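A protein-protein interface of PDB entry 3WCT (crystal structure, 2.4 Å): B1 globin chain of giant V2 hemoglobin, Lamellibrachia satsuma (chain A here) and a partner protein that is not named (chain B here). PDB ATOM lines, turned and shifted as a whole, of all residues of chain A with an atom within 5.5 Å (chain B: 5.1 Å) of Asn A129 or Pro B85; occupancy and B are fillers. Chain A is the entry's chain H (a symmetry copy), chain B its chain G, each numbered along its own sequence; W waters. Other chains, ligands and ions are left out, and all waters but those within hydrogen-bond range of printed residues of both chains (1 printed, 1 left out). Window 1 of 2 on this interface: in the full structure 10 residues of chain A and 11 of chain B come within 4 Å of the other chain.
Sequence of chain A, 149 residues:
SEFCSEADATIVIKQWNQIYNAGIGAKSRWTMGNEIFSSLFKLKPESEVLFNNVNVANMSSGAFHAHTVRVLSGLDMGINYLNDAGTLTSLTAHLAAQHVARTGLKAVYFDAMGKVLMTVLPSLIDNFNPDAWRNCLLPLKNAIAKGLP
Pro B85 touches Asn A129 (CG to OD1, 3.1 Å). Pro A130 touches Pro B85. Pro A130 touches Ser B86. Asn B89 touches Pro A130 (ND2 to CG, 3.8 Å). Asp A131 touches Pro B85.
Water W1 lies within hydrogen-bond range of the backbone carbonyl oxygen of Phe A128 (2.7 Å), the backbone NH of Ser B86 (2.9 Å) and the side-chain carboxylate of Asp B84 (2.9 Å).
The guanidinium group of Arg B10 lies within hydrogen-bond range of the backbone carbonyl oxygen of Leu B82, 3.1 Å away. The backbone carbonyl oxygen (O) of Pro B85 is in hydrogen-bond range of the side-chain amide nitrogen (ND2) of Asn B89, at 3.3 Å. The side-chain amide nitrogen (NE2) of Gln A15 lies within hydrogen-bond range of the backbone carbonyl oxygen (O) of Asn A127 (3.0 Å). The backbone NH of Asn A129 lies within hydrogen-bond range of the side-chain amide oxygen of Gln A15 (3.3 Å). The backbone NH (N) of Asp A131 lies within hydrogen-bond range of the side-chain amide oxygen (OD1) of Asn A129 (3.0 Å). The backbone NH (N) of Ala A132 lies within hydrogen-bond range of the side-chain amide oxygen (OD1) of Asn A129 (2.9 Å).
The guanidinium group (NH2) of Arg B10 is in salt-bridge range of the side-chain carboxylate (OD1) of Asp A131 (2.9 Å). OD1 of Asp B84 sits close to OD1 of Asn A127 (3.1 Å). OG of Ser B86 lies within hydrogen-bond range of O of Phe A128, 3.2 Å away. NE of Arg B139 is in salt-bridge range of OD1 of Asp A131 (2.7 Å).
Asn A129 touches just one residue of chain B: Pro B85 (3.1 Å). Pro B85 touches three residues of chain A. Printed residues of chain A within 4 Å of Asp B84: Asn A127 (3.1 Å). Of the printed residues of chain A, Arg B139 touches Asp A131. Leu B88 touches none of the printed residues of chain A. Ile A11 touches none of the printed residues of chain B. The nearest residue of chain B that does not touch Asn A129 is Ser B83 (4.5 Å).
Of the 11 printed residues of chain B, 6 touch a printed residue of chain A. Printed residues of chain B that touch a printed residue of chain A: Arg B10, Asp B84, Pro B85, Ser B86, Asn B89 and Arg B139. Of the 10 printed residues of chain A, 5 touch a printed residue of chain B. Among the printed residues, 9 pairs touch across the chains. Among the printed residues, Asp or Glu carboxylates within 4 Å of a Lys or Arg side-chain nitrogen of the other chain: Asp A131 with Arg B10 and Asp A131 with Arg B139.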
ATOM      1  N   ILE A  11     -27.018  33.007  18.061  1.00  0.00           N
ATOM      2  CA  ILE A  11     -27.295  31.979  17.069  1.00  0.00           C
ATOM      3  C   ILE A  11     -28.680  32.221  16.460  1.00  0.00           C
ATOM      4  O   ILE A  11     -28.823  32.239  15.241  1.00  0.00           O
ATOM      5  CB  ILE A  11     -27.192  30.574  17.708  1.00  0.00           C
ATOM      6  CG1 ILE A  11     -25.722  30.270  18.007  1.00  0.00           C
ATOM      7  CG2 ILE A  11     -27.744  29.523  16.789  1.00  0.00           C
ATOM      8  CD1 ILE A  11     -25.500  29.026  18.840  1.00  0.00           C
ATOM      9  N   GLN A  15     -29.457  33.165  12.653  1.00  0.00           N
ATOM     10  CA  GLN A  15     -30.223  32.221  11.853  1.00  0.00           C
ATOM     11  C   GLN A  15     -31.506  32.850  11.303  1.00  0.00           C
ATOM     12  O   GLN A  15     -31.941  32.529  10.198  1.00  0.00           O
ATOM     13  CB  GLN A  15     -30.533  30.957  12.664  1.00  0.00           C
ATOM     14  CG  GLN A  15     -29.318  30.084  12.886  1.00  0.00           C
ATOM     15  CD  GLN A  15     -29.674  28.680  13.362  1.00  0.00           C
ATOM     16  OE1 GLN A  15     -30.798  28.418  13.764  1.00  0.00           O
ATOM     17  NE2 GLN A  15     -28.704  27.778  13.328  1.00  0.00           N
ATOM     18  N   ASN A 127     -28.862  24.781   8.567  1.00  0.00           N
ATOM     19  CA  ASN A 127     -28.472  24.078   9.786  1.00  0.00           C
ATOM     20  C   ASN A 127     -29.109  24.639  11.056  1.00  0.00           C
ATOM     21  O   ASN A 127     -28.415  25.059  11.980  1.00  0.00           O
ATOM     22  CB  ASN A 127     -26.947  24.096   9.916  1.00  0.00           C
ATOM     23  CG  ASN A 127     -26.441  23.073  10.898  1.00  0.00           C
ATOM     24  OD1 ASN A 127     -26.983  21.964  10.990  1.00  0.00           O
ATOM     25  ND2 ASN A 127     -25.393  23.429  11.637  1.00  0.00           N
ATOM     26  N   PHE A 128     -30.435  24.635  11.088  1.00  0.00           N
ATOM     27  CA  PHE A 128     -31.212  25.109  12.230  1.00  0.00           C
ATOM     28  C   PHE A 128     -30.691  24.501  13.537  1.00  0.00           C
ATOM     29  O   PHE A 128     -30.232  23.368  13.554  1.00  0.00           O
ATOM     30  CB  PHE A 128     -32.664  24.694  12.026  1.00  0.00           C
ATOM     31  CG  PHE A 128     -33.606  25.234  13.047  1.00  0.00           C
ATOM     32  CD1 PHE A 128     -33.949  26.583  13.052  1.00  0.00           C
ATOM     33  CD2 PHE A 128     -34.197  24.383  13.973  1.00  0.00           C
ATOM     34  CE1 PHE A 128     -34.876  27.076  13.968  1.00  0.00           C
ATOM     35  CE2 PHE A 128     -35.121  24.860  14.887  1.00  0.00           C
ATOM     36  CZ  PHE A 128     -35.463  26.217  14.887  1.00  0.00           C
ATOM     37  N   ASN A 129     -30.774  25.261  14.623  1.00  0.00           N
ATOM     38  CA  ASN A 129     -30.337  24.809  15.948  1.00  0.00           C
ATOM     39  C   ASN A 129     -31.561  24.770  16.852  1.00  0.00           C
ATOM     40  O   ASN A 129     -31.918  25.774  17.472  1.00  0.00           O
ATOM     41  CB  ASN A 129     -29.318  25.785  16.548  1.00  0.00           C
ATOM     42  CG  ASN A 129     -28.743  25.296  17.880  1.00  0.00           C
ATOM     43  OD1 ASN A 129     -29.432  24.658  18.689  1.00  0.00           O
ATOM     44  ND2 ASN A 129     -27.476  25.616  18.116  1.00  0.00           N
ATOM     45  N   PRO A 130     -32.217  23.606  16.948  1.00  0.00           N
ATOM     46  CA  PRO A 130     -33.409  23.485  17.791  1.00  0.00           C
ATOM     47  C   PRO A 130     -33.241  23.847  19.279  1.00  0.00           C
ATOM     48  O   PRO A 130     -34.185  24.342  19.900  1.00  0.00           O
ATOM     49  CB  PRO A 130     -33.850  22.032  17.560  1.00  0.00           C
ATOM     50  CG  PRO A 130     -32.581  21.329  17.260  1.00  0.00           C
ATOM     51  CD  PRO A 130     -31.855  22.309  16.357  1.00  0.00           C
ATOM     52  N   ASP A 131     -32.059  23.634  19.850  1.00  0.00           N
ATOM     53  CA  ASP A 131     -31.849  23.954  21.265  1.00  0.00           C
ATOM     54  C   ASP A 131     -31.709  25.456  21.523  1.00  0.00           C
ATOM     55  O   ASP A 131     -32.323  25.983  22.454  1.00  0.00           O
ATOM     56  CB  ASP A 131     -30.634  23.198  21.817  1.00  0.00           C
ATOM     57  CG  ASP A 131     -30.919  21.720  22.030  1.00  0.00           C
ATOM     58  OD1 ASP A 131     -30.027  20.991  22.528  1.00  0.00           O
ATOM     59  OD2 ASP A 131     -32.039  21.276  21.704  1.00  0.00           O
ATOM     60  N   ALA A 132     -30.904  26.149  20.720  1.00  0.00           N
ATOM     61  CA  ALA A 132     -30.760  27.599  20.886  1.00  0.00           C
ATOM     62  C   ALA A 132     -32.137  28.226  20.682  1.00  0.00           C
ATOM     63  O   ALA A 132     -32.575  29.036  21.489  1.00  0.00           O
ATOM     64  CB  ALA A 132     -29.783  28.176  19.871  1.00  0.00           C
ATOM     65  N   TRP A 133     -32.820  27.846  19.602  1.00  0.00           N
ATOM     66  CA  TRP A 133     -34.147  28.390  19.337  1.00  0.00           C
ATOM     67  C   TRP A 133     -35.135  28.082  20.452  1.00  0.00           C
ATOM     68  O   TRP A 133     -35.916  28.945  20.824  1.00  0.00           O
ATOM     69  CB  TRP A 133     -34.688  27.893  18.001  1.00  0.00           C
ATOM     70  CG  TRP A 133     -34.160  28.694  16.849  1.00  0.00           C
ATOM     71  CD1 TRP A 133     -32.974  28.514  16.205  1.00  0.00           C
ATOM     72  CD2 TRP A 133     -34.787  29.831  16.232  1.00  0.00           C
ATOM     73  NE1 TRP A 133     -32.820  29.463  15.228  1.00  0.00           N
ATOM     74  CE2 TRP A 133     -33.914  30.288  15.226  1.00  0.00           C
ATOM     75  CE3 TRP A 133     -35.995  30.512  16.443  1.00  0.00           C
ATOM     76  CZ2 TRP A 133     -34.213  31.390  14.420  1.00  0.00           C
ATOM     77  CZ3 TRP A 133     -36.295  31.605  15.646  1.00  0.00           C
ATOM     78  CH2 TRP A 133     -35.402  32.037  14.645  1.00  0.00           C
ATOM     79  N   ARG A 134     -35.112  26.862  20.989  1.00  0.00           N
ATOM     80  CA  ARG A 134     -36.023  26.540  22.090  1.00  0.00           C
ATOM     81  C   ARG A 134     -35.695  27.429  23.290  1.00  0.00           C
ATOM     82  O   ARG A 134     -36.591  27.963  23.934  1.00  0.00           O
ATOM     83  CB  ARG A 134     -35.907  25.070  22.523  1.00  0.00           C
ATOM     84  CG  ARG A 134     -36.683  24.081  21.675  1.00  0.00           C
ATOM     85  CD  ARG A 134     -36.776  22.696  22.342  1.00  0.00           C
ATOM     86  NE  ARG A 134     -37.270  21.666  21.417  1.00  0.00           N
ATOM     87  CZ  ARG A 134     -36.502  20.909  20.625  1.00  0.00           C
ATOM     88  NH1 ARG A 134     -35.175  21.043  20.628  1.00  0.00           N
ATOM     89  NH2 ARG A 134     -37.066  20.014  19.818  1.00  0.00           N
ATOM     90  N   ARG B  10     -22.579  24.449  27.105  1.00  0.00           N
ATOM     91  CA  ARG B  10     -22.159  23.344  26.249  1.00  0.00           C
ATOM     92  C   ARG B  10     -20.655  23.397  26.014  1.00  0.00           C
ATOM     93  O   ARG B  10     -19.967  22.389  26.132  1.00  0.00           O
ATOM     94  CB  ARG B  10     -22.910  23.388  24.909  1.00  0.00           C
ATOM     95  CG  ARG B  10     -24.380  22.999  25.020  1.00  0.00           C
ATOM     96  CD  ARG B  10     -25.242  23.669  23.939  1.00  0.00           C
ATOM     97  NE  ARG B  10     -26.652  23.692  24.336  1.00  0.00           N
ATOM     98  CZ  ARG B  10     -27.556  22.789  23.973  1.00  0.00           C
ATOM     99  NH1 ARG B  10     -27.220  21.780  23.185  1.00  0.00           N
ATOM    100  NH2 ARG B  10     -28.793  22.883  24.420  1.00  0.00           N
ATOM    101  N   LEU B  81     -22.179  16.255  20.174  1.00  0.00           N
ATOM    102  CA  LEU B  81     -23.336  16.699  19.406  1.00  0.00           C
ATOM    103  C   LEU B  81     -24.140  17.830  20.051  1.00  0.00           C
ATOM    104  O   LEU B  81     -25.178  18.243  19.516  1.00  0.00           O
ATOM    105  CB  LEU B  81     -24.255  15.516  19.080  1.00  0.00           C
ATOM    106  CG  LEU B  81     -23.699  14.536  18.044  1.00  0.00           C
ATOM    107  CD1 LEU B  81     -24.694  13.400  17.850  1.00  0.00           C
ATOM    108  CD2 LEU B  81     -23.453  15.259  16.723  1.00  0.00           C
ATOM    109  N   LEU B  82     -23.669  18.333  21.196  1.00  0.00           N
ATOM    110  CA  LEU B  82     -24.354  19.452  21.844  1.00  0.00           C
ATOM    111  C   LEU B  82     -24.188  20.702  20.960  1.00  0.00           C
ATOM    112  O   LEU B  82     -24.907  21.680  21.118  1.00  0.00           O
ATOM    113  CB  LEU B  82     -23.764  19.724  23.232  1.00  0.00           C
ATOM    114  CG  LEU B  82     -24.123  18.790  24.393  1.00  0.00           C
ATOM    115  CD1 LEU B  82     -23.364  19.209  25.649  1.00  0.00           C
ATOM    116  CD2 LEU B  82     -25.613  18.860  24.663  1.00  0.00           C
ATOM    117  N   SER B  83     -23.223  20.644  20.041  1.00  0.00           N
ATOM    118  CA  SER B  83     -22.930  21.735  19.111  1.00  0.00           C
ATOM    119  C   SER B  83     -23.900  21.707  17.938  1.00  0.00           C
ATOM    120  O   SER B  83     -24.147  22.737  17.309  1.00  0.00           O
ATOM    121  CB  SER B  83     -21.507  21.620  18.562  1.00  0.00           C
ATOM    122  OG  SER B  83     -20.536  21.879  19.560  1.00  0.00           O
ATOM    123  N   ASP B  84     -24.417  20.521  17.627  1.00  0.00           N
ATOM    124  CA  ASP B  84     -25.392  20.371  16.549  1.00  0.00           C
ATOM    125  C   ASP B  84     -26.602  19.636  17.114  1.00  0.00           C
ATOM    126  O   ASP B  84     -26.719  18.420  16.985  1.00  0.00           O
ATOM    127  CB  ASP B  84     -24.804  19.595  15.355  1.00  0.00           C
ATOM    128  CG  ASP B  84     -25.741  19.602  14.133  1.00  0.00           C
ATOM    129  OD1 ASP B  84     -26.188  20.704  13.718  1.00  0.00           O
ATOM    130  OD2 ASP B  84     -26.032  18.512  13.587  1.00  0.00           O
ATOM    131  N   PRO B  85     -27.520  20.376  17.755  1.00  0.00           N
ATOM    132  CA  PRO B  85     -28.732  19.818  18.359  1.00  0.00           C
ATOM    133  C   PRO B  85     -29.654  18.963  17.471  1.00  0.00           C
ATOM    134  O   PRO B  85     -30.231  17.980  17.953  1.00  0.00           O
ATOM    135  CB  PRO B  85     -29.414  21.057  18.924  1.00  0.00           C
ATOM    136  CG  PRO B  85     -28.245  21.856  19.389  1.00  0.00           C
ATOM    137  CD  PRO B  85     -27.362  21.784  18.153  1.00  0.00           C
ATOM    138  N   SER B  86     -29.797  19.329  16.198  1.00  0.00           N
ATOM    139  CA  SER B  86     -30.636  18.566  15.268  1.00  0.00           C
ATOM    140  C   SER B  86     -30.203  17.123  15.261  1.00  0.00           C
ATOM    141  O   SER B  86     -31.021  16.223  15.395  1.00  0.00           O
ATOM    142  CB  SER B  86     -30.508  19.091  13.837  1.00  0.00           C
ATOM    143  OG  SER B  86     -31.195  20.313  13.677  1.00  0.00           O
ATOM    144  N   THR B  87     -28.905  16.911  15.075  1.00  0.00           N
ATOM    145  CA  THR B  87     -28.341  15.578  15.040  1.00  0.00           C
ATOM    146  C   THR B  87     -28.318  14.951  16.430  1.00  0.00           C
ATOM    147  O   THR B  87     -28.407  13.731  16.564  1.00  0.00           O
ATOM    148  CB  THR B  87     -26.920  15.602  14.479  1.00  0.00           C
ATOM    149  OG1 THR B  87     -26.961  16.097  13.140  1.00  0.00           O
ATOM    150  CG2 THR B  87     -26.322  14.208  14.473  1.00  0.00           C
ATOM    151  N   LEU B  88     -28.190  15.788  17.458  1.00  0.00           N
ATOM    152  CA  LEU B  88     -28.176  15.291  18.823  1.00  0.00           C
ATOM    153  C   LEU B  88     -29.504  14.579  19.085  1.00  0.00           C
ATOM    154  O   LEU B  88     -29.529  13.467  19.613  1.00  0.00           O
ATOM    155  CB  LEU B  88     -28.015  16.439  19.821  1.00  0.00           C
ATOM    156  CG  LEU B  88     -28.363  16.086  21.282  1.00  0.00           C
ATOM    157  CD1 LEU B  88     -27.401  15.049  21.841  1.00  0.00           C
ATOM    158  CD2 LEU B  88     -28.308  17.335  22.111  1.00  0.00           C
ATOM    159  N   ASN B  89     -30.604  15.219  18.694  1.00  0.00           N
ATOM    160  CA  ASN B  89     -31.919  14.631  18.929  1.00  0.00           C
ATOM    161  C   ASN B  89     -32.056  13.254  18.327  1.00  0.00           C
ATOM    162  O   ASN B  89     -32.646  12.377  18.934  1.00  0.00           O
ATOM    163  CB  ASN B  89     -33.034  15.557  18.426  1.00  0.00           C
ATOM    164  CG  ASN B  89     -33.184  16.779  19.297  1.00  0.00           C
ATOM    165  OD1 ASN B  89     -33.060  16.689  20.516  1.00  0.00           O
ATOM    166  ND2 ASN B  89     -33.448  17.925  18.689  1.00  0.00           N
ATOM    167  N   ARG B 139     -30.103  17.573  30.068  1.00  0.00           N
ATOM    168  CA  ARG B 139     -30.635  17.815  28.735  1.00  0.00           C
ATOM    169  C   ARG B 139     -30.376  16.584  27.872  1.00  0.00           C
ATOM    170  O   ARG B 139     -31.159  16.262  26.980  1.00  0.00           O
ATOM    171  CB  ARG B 139     -29.959  19.040  28.115  1.00  0.00           C
ATOM    172  CG  ARG B 139     -29.890  19.015  26.588  1.00  0.00           C
ATOM    173  CD  ARG B 139     -31.160  19.535  25.962  1.00  0.00           C
ATOM    174  NE  ARG B 139     -31.111  19.483  24.504  1.00  0.00           N
ATOM    175  CZ  ARG B 139     -31.361  18.400  23.775  1.00  0.00           C
ATOM    176  NH1 ARG B 139     -31.675  17.251  24.364  1.00  0.00           N
ATOM    177  NH2 ARG B 139     -31.348  18.482  22.454  1.00  0.00           N
HETATM  178  O   HOH W   1     -28.638  21.610  14.921  1.00  0.00           O
